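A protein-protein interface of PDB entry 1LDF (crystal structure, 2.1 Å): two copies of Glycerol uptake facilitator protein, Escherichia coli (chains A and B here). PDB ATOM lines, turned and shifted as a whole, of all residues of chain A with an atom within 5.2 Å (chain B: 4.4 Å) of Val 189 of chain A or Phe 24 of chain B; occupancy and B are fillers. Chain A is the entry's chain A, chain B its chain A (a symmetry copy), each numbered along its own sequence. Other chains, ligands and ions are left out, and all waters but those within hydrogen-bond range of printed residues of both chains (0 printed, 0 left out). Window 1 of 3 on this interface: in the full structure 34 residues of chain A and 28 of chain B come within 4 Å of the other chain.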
ATOM      1  N   TRP A  42       7.063  -4.033  17.857  1.00  0.00           N
ATOM      2  CA  TRP A  42       7.433  -3.107  16.793  1.00  0.00           C
ATOM      3  C   TRP A  42       7.184  -3.717  15.411  1.00  0.00           C
ATOM      4  O   TRP A  42       6.712  -3.033  14.503  1.00  0.00           O
ATOM      5  CB  TRP A  42       8.910  -2.697  16.918  1.00  0.00           C
ATOM      6  CG  TRP A  42       9.496  -2.135  15.641  1.00  0.00           C
ATOM      7  CD1 TRP A  42      10.396  -2.748  14.818  1.00  0.00           C
ATOM      8  CD2 TRP A  42       9.175  -0.883  15.023  1.00  0.00           C
ATOM      9  NE1 TRP A  42      10.653  -1.957  13.722  1.00  0.00           N
ATOM     10  CE2 TRP A  42       9.915  -0.806  13.822  1.00  0.00           C
ATOM     11  CE3 TRP A  42       8.328   0.181  15.365  1.00  0.00           C
ATOM     12  CZ2 TRP A  42       9.837   0.295  12.960  1.00  0.00           C
ATOM     13  CZ3 TRP A  42       8.249   1.277  14.506  1.00  0.00           C
ATOM     14  CH2 TRP A  42       8.999   1.323  13.318  1.00  0.00           C
ATOM     15  N   ILE A 158      -3.575  12.547  17.898  1.00  0.00           N
ATOM     16  CA  ILE A 158      -2.192  12.623  17.433  1.00  0.00           C
ATOM     17  C   ILE A 158      -2.136  12.198  15.969  1.00  0.00           C
ATOM     18  O   ILE A 158      -1.428  12.802  15.161  1.00  0.00           O
ATOM     19  CB  ILE A 158      -1.273  11.692  18.262  1.00  0.00           C
ATOM     20  CG1 ILE A 158      -1.061  12.285  19.656  1.00  0.00           C
ATOM     21  CG2 ILE A 158       0.053  11.478  17.548  1.00  0.00           C
ATOM     22  CD1 ILE A 158      -0.215  11.416  20.573  1.00  0.00           C
ATOM     23  N   LEU A 185       4.740   5.327   8.830  1.00  0.00           N
ATOM     24  CA  LEU A 185       5.726   5.247   9.905  1.00  0.00           C
ATOM     25  C   LEU A 185       5.135   5.832  11.184  1.00  0.00           C
ATOM     26  O   LEU A 185       5.441   5.371  12.293  1.00  0.00           O
ATOM     27  CB  LEU A 185       7.014   5.978   9.518  1.00  0.00           C
ATOM     28  CG  LEU A 185       7.846   5.270   8.443  1.00  0.00           C
ATOM     29  CD1 LEU A 185       9.132   6.056   8.215  1.00  0.00           C
ATOM     30  CD2 LEU A 185       8.174   3.825   8.875  1.00  0.00           C
ATOM     31  N   LEU A 186       4.282   6.840  11.022  1.00  0.00           N
ATOM     32  CA  LEU A 186       3.616   7.472  12.157  1.00  0.00           C
ATOM     33  C   LEU A 186       2.714   6.449  12.849  1.00  0.00           C
ATOM     34  O   LEU A 186       2.707   6.327  14.075  1.00  0.00           O
ATOM     35  CB  LEU A 186       2.753   8.640  11.682  1.00  0.00           C
ATOM     36  CG  LEU A 186       1.712   9.139  12.687  1.00  0.00           C
ATOM     37  CD1 LEU A 186       2.416   9.835  13.847  1.00  0.00           C
ATOM     38  CD2 LEU A 186       0.738  10.087  11.992  1.00  0.00           C
ATOM     39  N   ILE A 187       1.938   5.731  12.044  1.00  0.00           N
ATOM     40  CA  ILE A 187       1.023   4.721  12.555  1.00  0.00           C
ATOM     41  C   ILE A 187       1.811   3.627  13.258  1.00  0.00           C
ATOM     42  O   ILE A 187       1.363   3.079  14.260  1.00  0.00           O
ATOM     43  CB  ILE A 187       0.171   4.151  11.401  1.00  0.00           C
ATOM     44  CG1 ILE A 187      -0.845   5.220  10.979  1.00  0.00           C
ATOM     45  CG2 ILE A 187      -0.534   2.853  11.821  1.00  0.00           C
ATOM     46  CD1 ILE A 187      -1.555   4.927   9.683  1.00  0.00           C
ATOM     47  N   ALA A 188       3.001   3.340  12.741  1.00  0.00           N
ATOM     48  CA  ALA A 188       3.873   2.340  13.324  1.00  0.00           C
ATOM     49  C   ALA A 188       4.311   2.728  14.745  1.00  0.00           C
ATOM     50  O   ALA A 188       4.251   1.901  15.656  1.00  0.00           O
ATOM     51  CB  ALA A 188       5.095   2.133  12.429  1.00  0.00           C
ATOM     52  N   VAL A 189       4.736   3.977  14.947  1.00  0.00           N
ATOM     53  CA  VAL A 189       5.179   4.393  16.278  1.00  0.00           C
ATOM     54  C   VAL A 189       4.022   4.530  17.258  1.00  0.00           C
ATOM     55  O   VAL A 189       4.199   4.315  18.462  1.00  0.00           O
ATOM     56  CB  VAL A 189       6.035   5.709  16.249  1.00  0.00           C
ATOM     57  CG1 VAL A 189       7.264   5.496  15.378  1.00  0.00           C
ATOM     58  CG2 VAL A 189       5.224   6.885  15.750  1.00  0.00           C
ATOM     59  N   ILE A 190       2.839   4.879  16.757  1.00  0.00           N
ATOM     60  CA  ILE A 190       1.665   4.970  17.624  1.00  0.00           C
ATOM     61  C   ILE A 190       1.321   3.544  18.089  1.00  0.00           C
ATOM     62  O   ILE A 190       1.081   3.309  19.266  1.00  0.00           O
ATOM     63  CB  ILE A 190       0.434   5.533  16.883  1.00  0.00           C
ATOM     64  CG1 ILE A 190       0.641   7.018  16.556  1.00  0.00           C
ATOM     65  CG2 ILE A 190      -0.817   5.340  17.729  1.00  0.00           C
ATOM     66  CD1 ILE A 190      -0.494   7.619  15.763  1.00  0.00           C
ATOM     67  N   GLY A 191       1.311   2.598  17.154  1.00  0.00           N
ATOM     68  CA  GLY A 191       0.994   1.226  17.505  1.00  0.00           C
ATOM     69  C   GLY A 191       1.993   0.563  18.445  1.00  0.00           C
ATOM     70  O   GLY A 191       1.610  -0.244  19.297  1.00  0.00           O
ATOM     71  N   ALA A 192       3.271   0.901  18.296  1.00  0.00           N
ATOM     72  CA  ALA A 192       4.321   0.313  19.119  1.00  0.00           C
ATOM     73  C   ALA A 192       4.389   0.888  20.533  1.00  0.00           C
ATOM     74  O   ALA A 192       4.731   0.181  21.489  1.00  0.00           O
ATOM     75  CB  ALA A 192       5.673   0.488  18.423  1.00  0.00           C
ATOM     76  N   SER A 193       4.062   2.168  20.668  1.00  0.00           N
ATOM     77  CA  SER A 193       4.117   2.835  21.963  1.00  0.00           C
ATOM     78  C   SER A 193       2.843   2.718  22.798  1.00  0.00           C
ATOM     79  O   SER A 193       2.883   2.842  24.027  1.00  0.00           O
ATOM     80  CB  SER A 193       4.445   4.317  21.755  1.00  0.00           C
ATOM     81  OG  SER A 193       3.393   4.978  21.062  1.00  0.00           O
ATOM     82  N   MET A 194       1.713   2.486  22.136  1.00  0.00           N
ATOM     83  CA  MET A 194       0.439   2.400  22.842  1.00  0.00           C
ATOM     84  C   MET A 194      -0.339   1.118  22.594  1.00  0.00           C
ATOM     85  O   MET A 194      -1.323   0.854  23.273  1.00  0.00           O
ATOM     86  CB  MET A 194      -0.439   3.595  22.457  1.00  0.00           C
ATOM     87  CG  MET A 194       0.079   4.942  22.939  1.00  0.00           C
ATOM     88  SD  MET A 194      -0.091   5.152  24.723  1.00  0.00           S
ATOM     89  CE  MET A 194       1.517   5.851  25.137  1.00  0.00           C
ATOM     90  N   LEU B  20       5.787  15.411  22.116  1.00  0.00           N
ATOM     91  CA  LEU B  20       5.479  14.314  21.199  1.00  0.00           C
ATOM     92  C   LEU B  20       6.557  13.228  21.247  1.00  0.00           C
ATOM     93  O   LEU B  20       6.250  12.047  21.396  1.00  0.00           O
ATOM     94  CB  LEU B  20       5.370  14.831  19.760  1.00  0.00           C
ATOM     95  CG  LEU B  20       4.252  14.305  18.849  1.00  0.00           C
ATOM     96  CD1 LEU B  20       4.818  14.090  17.444  1.00  0.00           C
ATOM     97  CD2 LEU B  20       3.661  13.009  19.388  1.00  0.00           C
ATOM     98  N   LEU B  21       7.817  13.634  21.119  1.00  0.00           N
ATOM     99  CA  LEU B  21       8.916  12.679  21.129  1.00  0.00           C
ATOM    100  C   LEU B  21       9.009  11.918  22.455  1.00  0.00           C
ATOM    101  O   LEU B  21       9.475  10.785  22.485  1.00  0.00           O
ATOM    102  CB  LEU B  21      10.243  13.381  20.784  1.00  0.00           C
ATOM    103  CG  LEU B  21      10.901  14.418  21.701  1.00  0.00           C
ATOM    104  CD1 LEU B  21      11.837  13.715  22.692  1.00  0.00           C
ATOM    105  CD2 LEU B  21      11.715  15.413  20.851  1.00  0.00           C
ATOM    106  N   ILE B  22       8.551  12.530  23.544  1.00  0.00           N
ATOM    107  CA  ILE B  22       8.567  11.871  24.852  1.00  0.00           C
ATOM    108  C   ILE B  22       7.406  10.874  24.931  1.00  0.00           C
ATOM    109  O   ILE B  22       7.545   9.785  25.495  1.00  0.00           O
ATOM    110  CB  ILE B  22       8.444  12.908  26.003  1.00  0.00           C
ATOM    111  CG1 ILE B  22       9.794  13.589  26.228  1.00  0.00           C
ATOM    112  CG2 ILE B  22       7.952  12.245  27.284  1.00  0.00           C
ATOM    113  CD1 ILE B  22      10.895  12.651  26.671  1.00  0.00           C
ATOM    114  N   PHE B  23       6.266  11.253  24.358  1.00  0.00           N
ATOM    115  CA  PHE B  23       5.080  10.401  24.343  1.00  0.00           C
ATOM    116  C   PHE B  23       5.423   9.047  23.716  1.00  0.00           C
ATOM    117  O   PHE B  23       5.178   8.001  24.311  1.00  0.00           O
ATOM    118  CB  PHE B  23       3.961  11.074  23.535  1.00  0.00           C
ATOM    119  CG  PHE B  23       2.682  10.275  23.474  1.00  0.00           C
ATOM    120  CD1 PHE B  23       1.768  10.319  24.520  1.00  0.00           C
ATOM    121  CD2 PHE B  23       2.391   9.485  22.361  1.00  0.00           C
ATOM    122  CE1 PHE B  23       0.579   9.592  24.462  1.00  0.00           C
ATOM    123  CE2 PHE B  23       1.202   8.751  22.292  1.00  0.00           C
ATOM    124  CZ  PHE B  23       0.294   8.806  23.343  1.00  0.00           C
ATOM    125  N   PHE B  24       5.991   9.080  22.516  1.00  0.00           N
ATOM    126  CA  PHE B  24       6.370   7.864  21.806  1.00  0.00           C
ATOM    127  C   PHE B  24       7.506   7.123  22.506  1.00  0.00           C
ATOM    128  O   PHE B  24       7.453   5.903  22.675  1.00  0.00           O
ATOM    129  CB  PHE B  24       6.809   8.204  20.379  1.00  0.00           C
ATOM    130  CG  PHE B  24       5.706   8.744  19.509  1.00  0.00           C
ATOM    131  CD1 PHE B  24       5.934   9.845  18.684  1.00  0.00           C
ATOM    132  CD2 PHE B  24       4.456   8.130  19.479  1.00  0.00           C
ATOM    133  CE1 PHE B  24       4.932  10.328  17.840  1.00  0.00           C
ATOM    134  CE2 PHE B  24       3.447   8.602  18.642  1.00  0.00           C
ATOM    135  CZ  PHE B  24       3.686   9.705  17.817  1.00  0.00           C
ATOM    136  N   GLY B  25       8.533   7.869  22.899  1.00  0.00           N
ATOM    137  CA  GLY B  25       9.686   7.279  23.555  1.00  0.00           C
ATOM    138  C   GLY B  25       9.399   6.614  24.883  1.00  0.00           C
ATOM    139  O   GLY B  25       9.719   5.443  25.077  1.00  0.00           O
ATOM    140  N   VAL B  26       8.799   7.364  25.800  1.00  0.00           N
ATOM    141  CA  VAL B  26       8.457   6.848  27.122  1.00  0.00           C
ATOM    142  C   VAL B  26       7.343   5.815  26.968  1.00  0.00           C
ATOM    143  O   VAL B  26       7.270   4.834  27.718  1.00  0.00           O
ATOM    144  CB  VAL B  26       7.995   8.006  28.047  1.00  0.00           C
ATOM    145  CG1 VAL B  26       7.552   7.474  29.403  1.00  0.00           C
ATOM    146  CG2 VAL B  26       9.135   9.011  28.204  1.00  0.00           C
ATOM    147  N   GLY B  27       6.479   6.037  25.979  1.00  0.00           N
ATOM    148  CA  GLY B  27       5.396   5.102  25.734  1.00  0.00           C
ATOM    149  C   GLY B  27       5.883   3.682  25.462  1.00  0.00           C
ATOM    150  O   GLY B  27       5.426   2.731  26.116  1.00  0.00           O
ATOM    151  N   CYS B  28       6.808   3.514  24.515  1.00  0.00           N
ATOM    152  CA  CYS B  28       7.284   2.170  24.201  1.00  0.00           C
ATOM    153  C   CYS B  28       8.101   1.534  25.327  1.00  0.00           C
ATOM    154  O   CYS B  28       8.090   0.313  25.485  1.00  0.00           O
ATOM    155  CB  CYS B  28       8.064   2.150  22.871  1.00  0.00           C
ATOM    156  SG  CYS B  28       9.688   2.969  22.813  1.00  0.00           S
ATOM    157  N   ILE B  47      12.024   3.305  17.353  1.00  0.00           N
ATOM    158  CA  ILE B  47      10.734   3.902  17.676  1.00  0.00           C
ATOM    159  C   ILE B  47      10.956   5.323  18.211  1.00  0.00           C
ATOM    160  O   ILE B  47      10.204   6.255  17.882  1.00  0.00           O
ATOM    161  CB  ILE B  47       9.982   3.084  18.754  1.00  0.00           C
ATOM    162  CG1 ILE B  47       9.544   1.733  18.187  1.00  0.00           C
ATOM    163  CG2 ILE B  47       8.766   3.868  19.248  1.00  0.00           C
ATOM    164  CD1 ILE B  47       9.172   0.702  19.271  1.00  0.00           C
ATOM    165  N   LEU B  50      12.275   7.609  15.153  1.00  0.00           N
ATOM    166  CA  LEU B  50      11.183   7.949  14.238  1.00  0.00           C
ATOM    167  C   LEU B  50      10.197   8.901  14.909  1.00  0.00           C
ATOM    168  O   LEU B  50       9.604   9.757  14.249  1.00  0.00           O
ATOM    169  CB  LEU B  50      10.447   6.689  13.773  1.00  0.00           C
ATOM    170  CG  LEU B  50      11.250   5.813  12.805  1.00  0.00           C
ATOM    171  CD1 LEU B  50      10.468   4.547  12.486  1.00  0.00           C
ATOM    172  CD2 LEU B  50      11.546   6.603  11.518  1.00  0.00           C
ATOM    173  N   GLY B  51      10.024   8.749  16.216  1.00  0.00           N
ATOM    174  CA  GLY B  51       9.127   9.627  16.940  1.00  0.00           C
ATOM    175  C   GLY B  51       9.662  11.047  16.906  1.00  0.00           C
ATOM    176  O   GLY B  51       8.897  12.013  16.824  1.00  0.00           O
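The backbone carbonyl oxygen of Ser 193 of chain A lies close to the backbone carbonyl oxygen of Gly 27 of chain B (3.3 Å).
The backbone carbonyl oxygen (O) of Gly 25 of chain B lies within hydrogen-bond range of the side-chain sulfur (SG) of Cys 28 of chain B, at 3.4 Å.
OG of Ser 193 of chain A lies within hydrogen-bond range of O of Ile 190 of chain A (3.4 Å).
The backbone carbonyl oxygen (O) of Phe 24 of chain B lies within hydrogen-bond range of the side-chain sulfur (SG) of Cys 28 of chain B, 3.7 Å away.
OG of Ser 193 of chain A lies within hydrogen-bond range of O of Val 189 of chain A (2.8 Å).
Trp 42 of chain A touches Ile 47 of chain B.
Leu 50 of chain B touches Trp 42 of chain A.
Val 189 of chain A touches Ile 47 of chain B (CG1 to O, 3.9 Å).
Val 189 of chain A touches Leu 50 of chain B (CG1 to CB, 3.8 Å).
Phe 24 of chain B touches Ile 190 of chain A.
Ala 192 of chain A touches Ile 47 of chain B.
Ser 193 of chain A touches Phe 24 of chain B (CB to O, 3.5 Å).
CB of Ser 193 of chain A touches N of Cys 28 of chain B (3.7 Å).
Met 194 of chain A touches Phe 23 of chain B.
CA of Gly 27 of chain B touches CE of Met 194 of chain A (3.996 Å).
Of chain B, only Phe 24 (3.8 Å), Ile 47 (3.9 Å) and Leu 50 (3.8 Å) come within 4 Å of Val 189 of chain A.
Of chain A, only Val 189 (3.8 Å), Ile 190 (3.8 Å) and Ser 193 (3.5 Å) come within 4 Å of Phe 24 of chain B.
Of the printed residues of chain B, Trp 42 of chain A touches Ile 47 (3.4 Å) and Leu 50 (3.6 Å).
Of the printed residues of chain B, Ile 158 of chain A touches Phe 23.
Leu 185 of chain A touches none of the printed residues of chain B.
The nearest printed residue of chain A that does not touch Cys 28 of chain B is Ala 192 of chain A (4.1 Å).
Hydrophobic or aromatic side chains of chain A within 4 Å of the printed part of chain B: Trp 42, Ile 158, Val 189, Ile 190, Ala 192 and Met 194.
Of the 12 printed residues of chain B, 6 touch a printed residue of chain A.
Printed residues of chain B that touch a printed residue of chain A: Phe 23, Phe 24, Gly 27, Cys 28, Ile 47 and Leu 50.
Hydrophobic or aromatic side chains of chain B within 4 Å of the printed part of chain A: Phe 23, Phe 24, Ile 47 and Leu 50.
Among the printed residues, 13 pairs touch across the chains.
Among the printed residues, no Asp or Glu carboxylate lies within 4 Å of a Lys or Arg side-chain nitrogen of the other chain.
No position is printed for both chains.
Of the 13 pairs that touch across the chains among the printed residues, none has its exchanged pair printed and touching as well.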
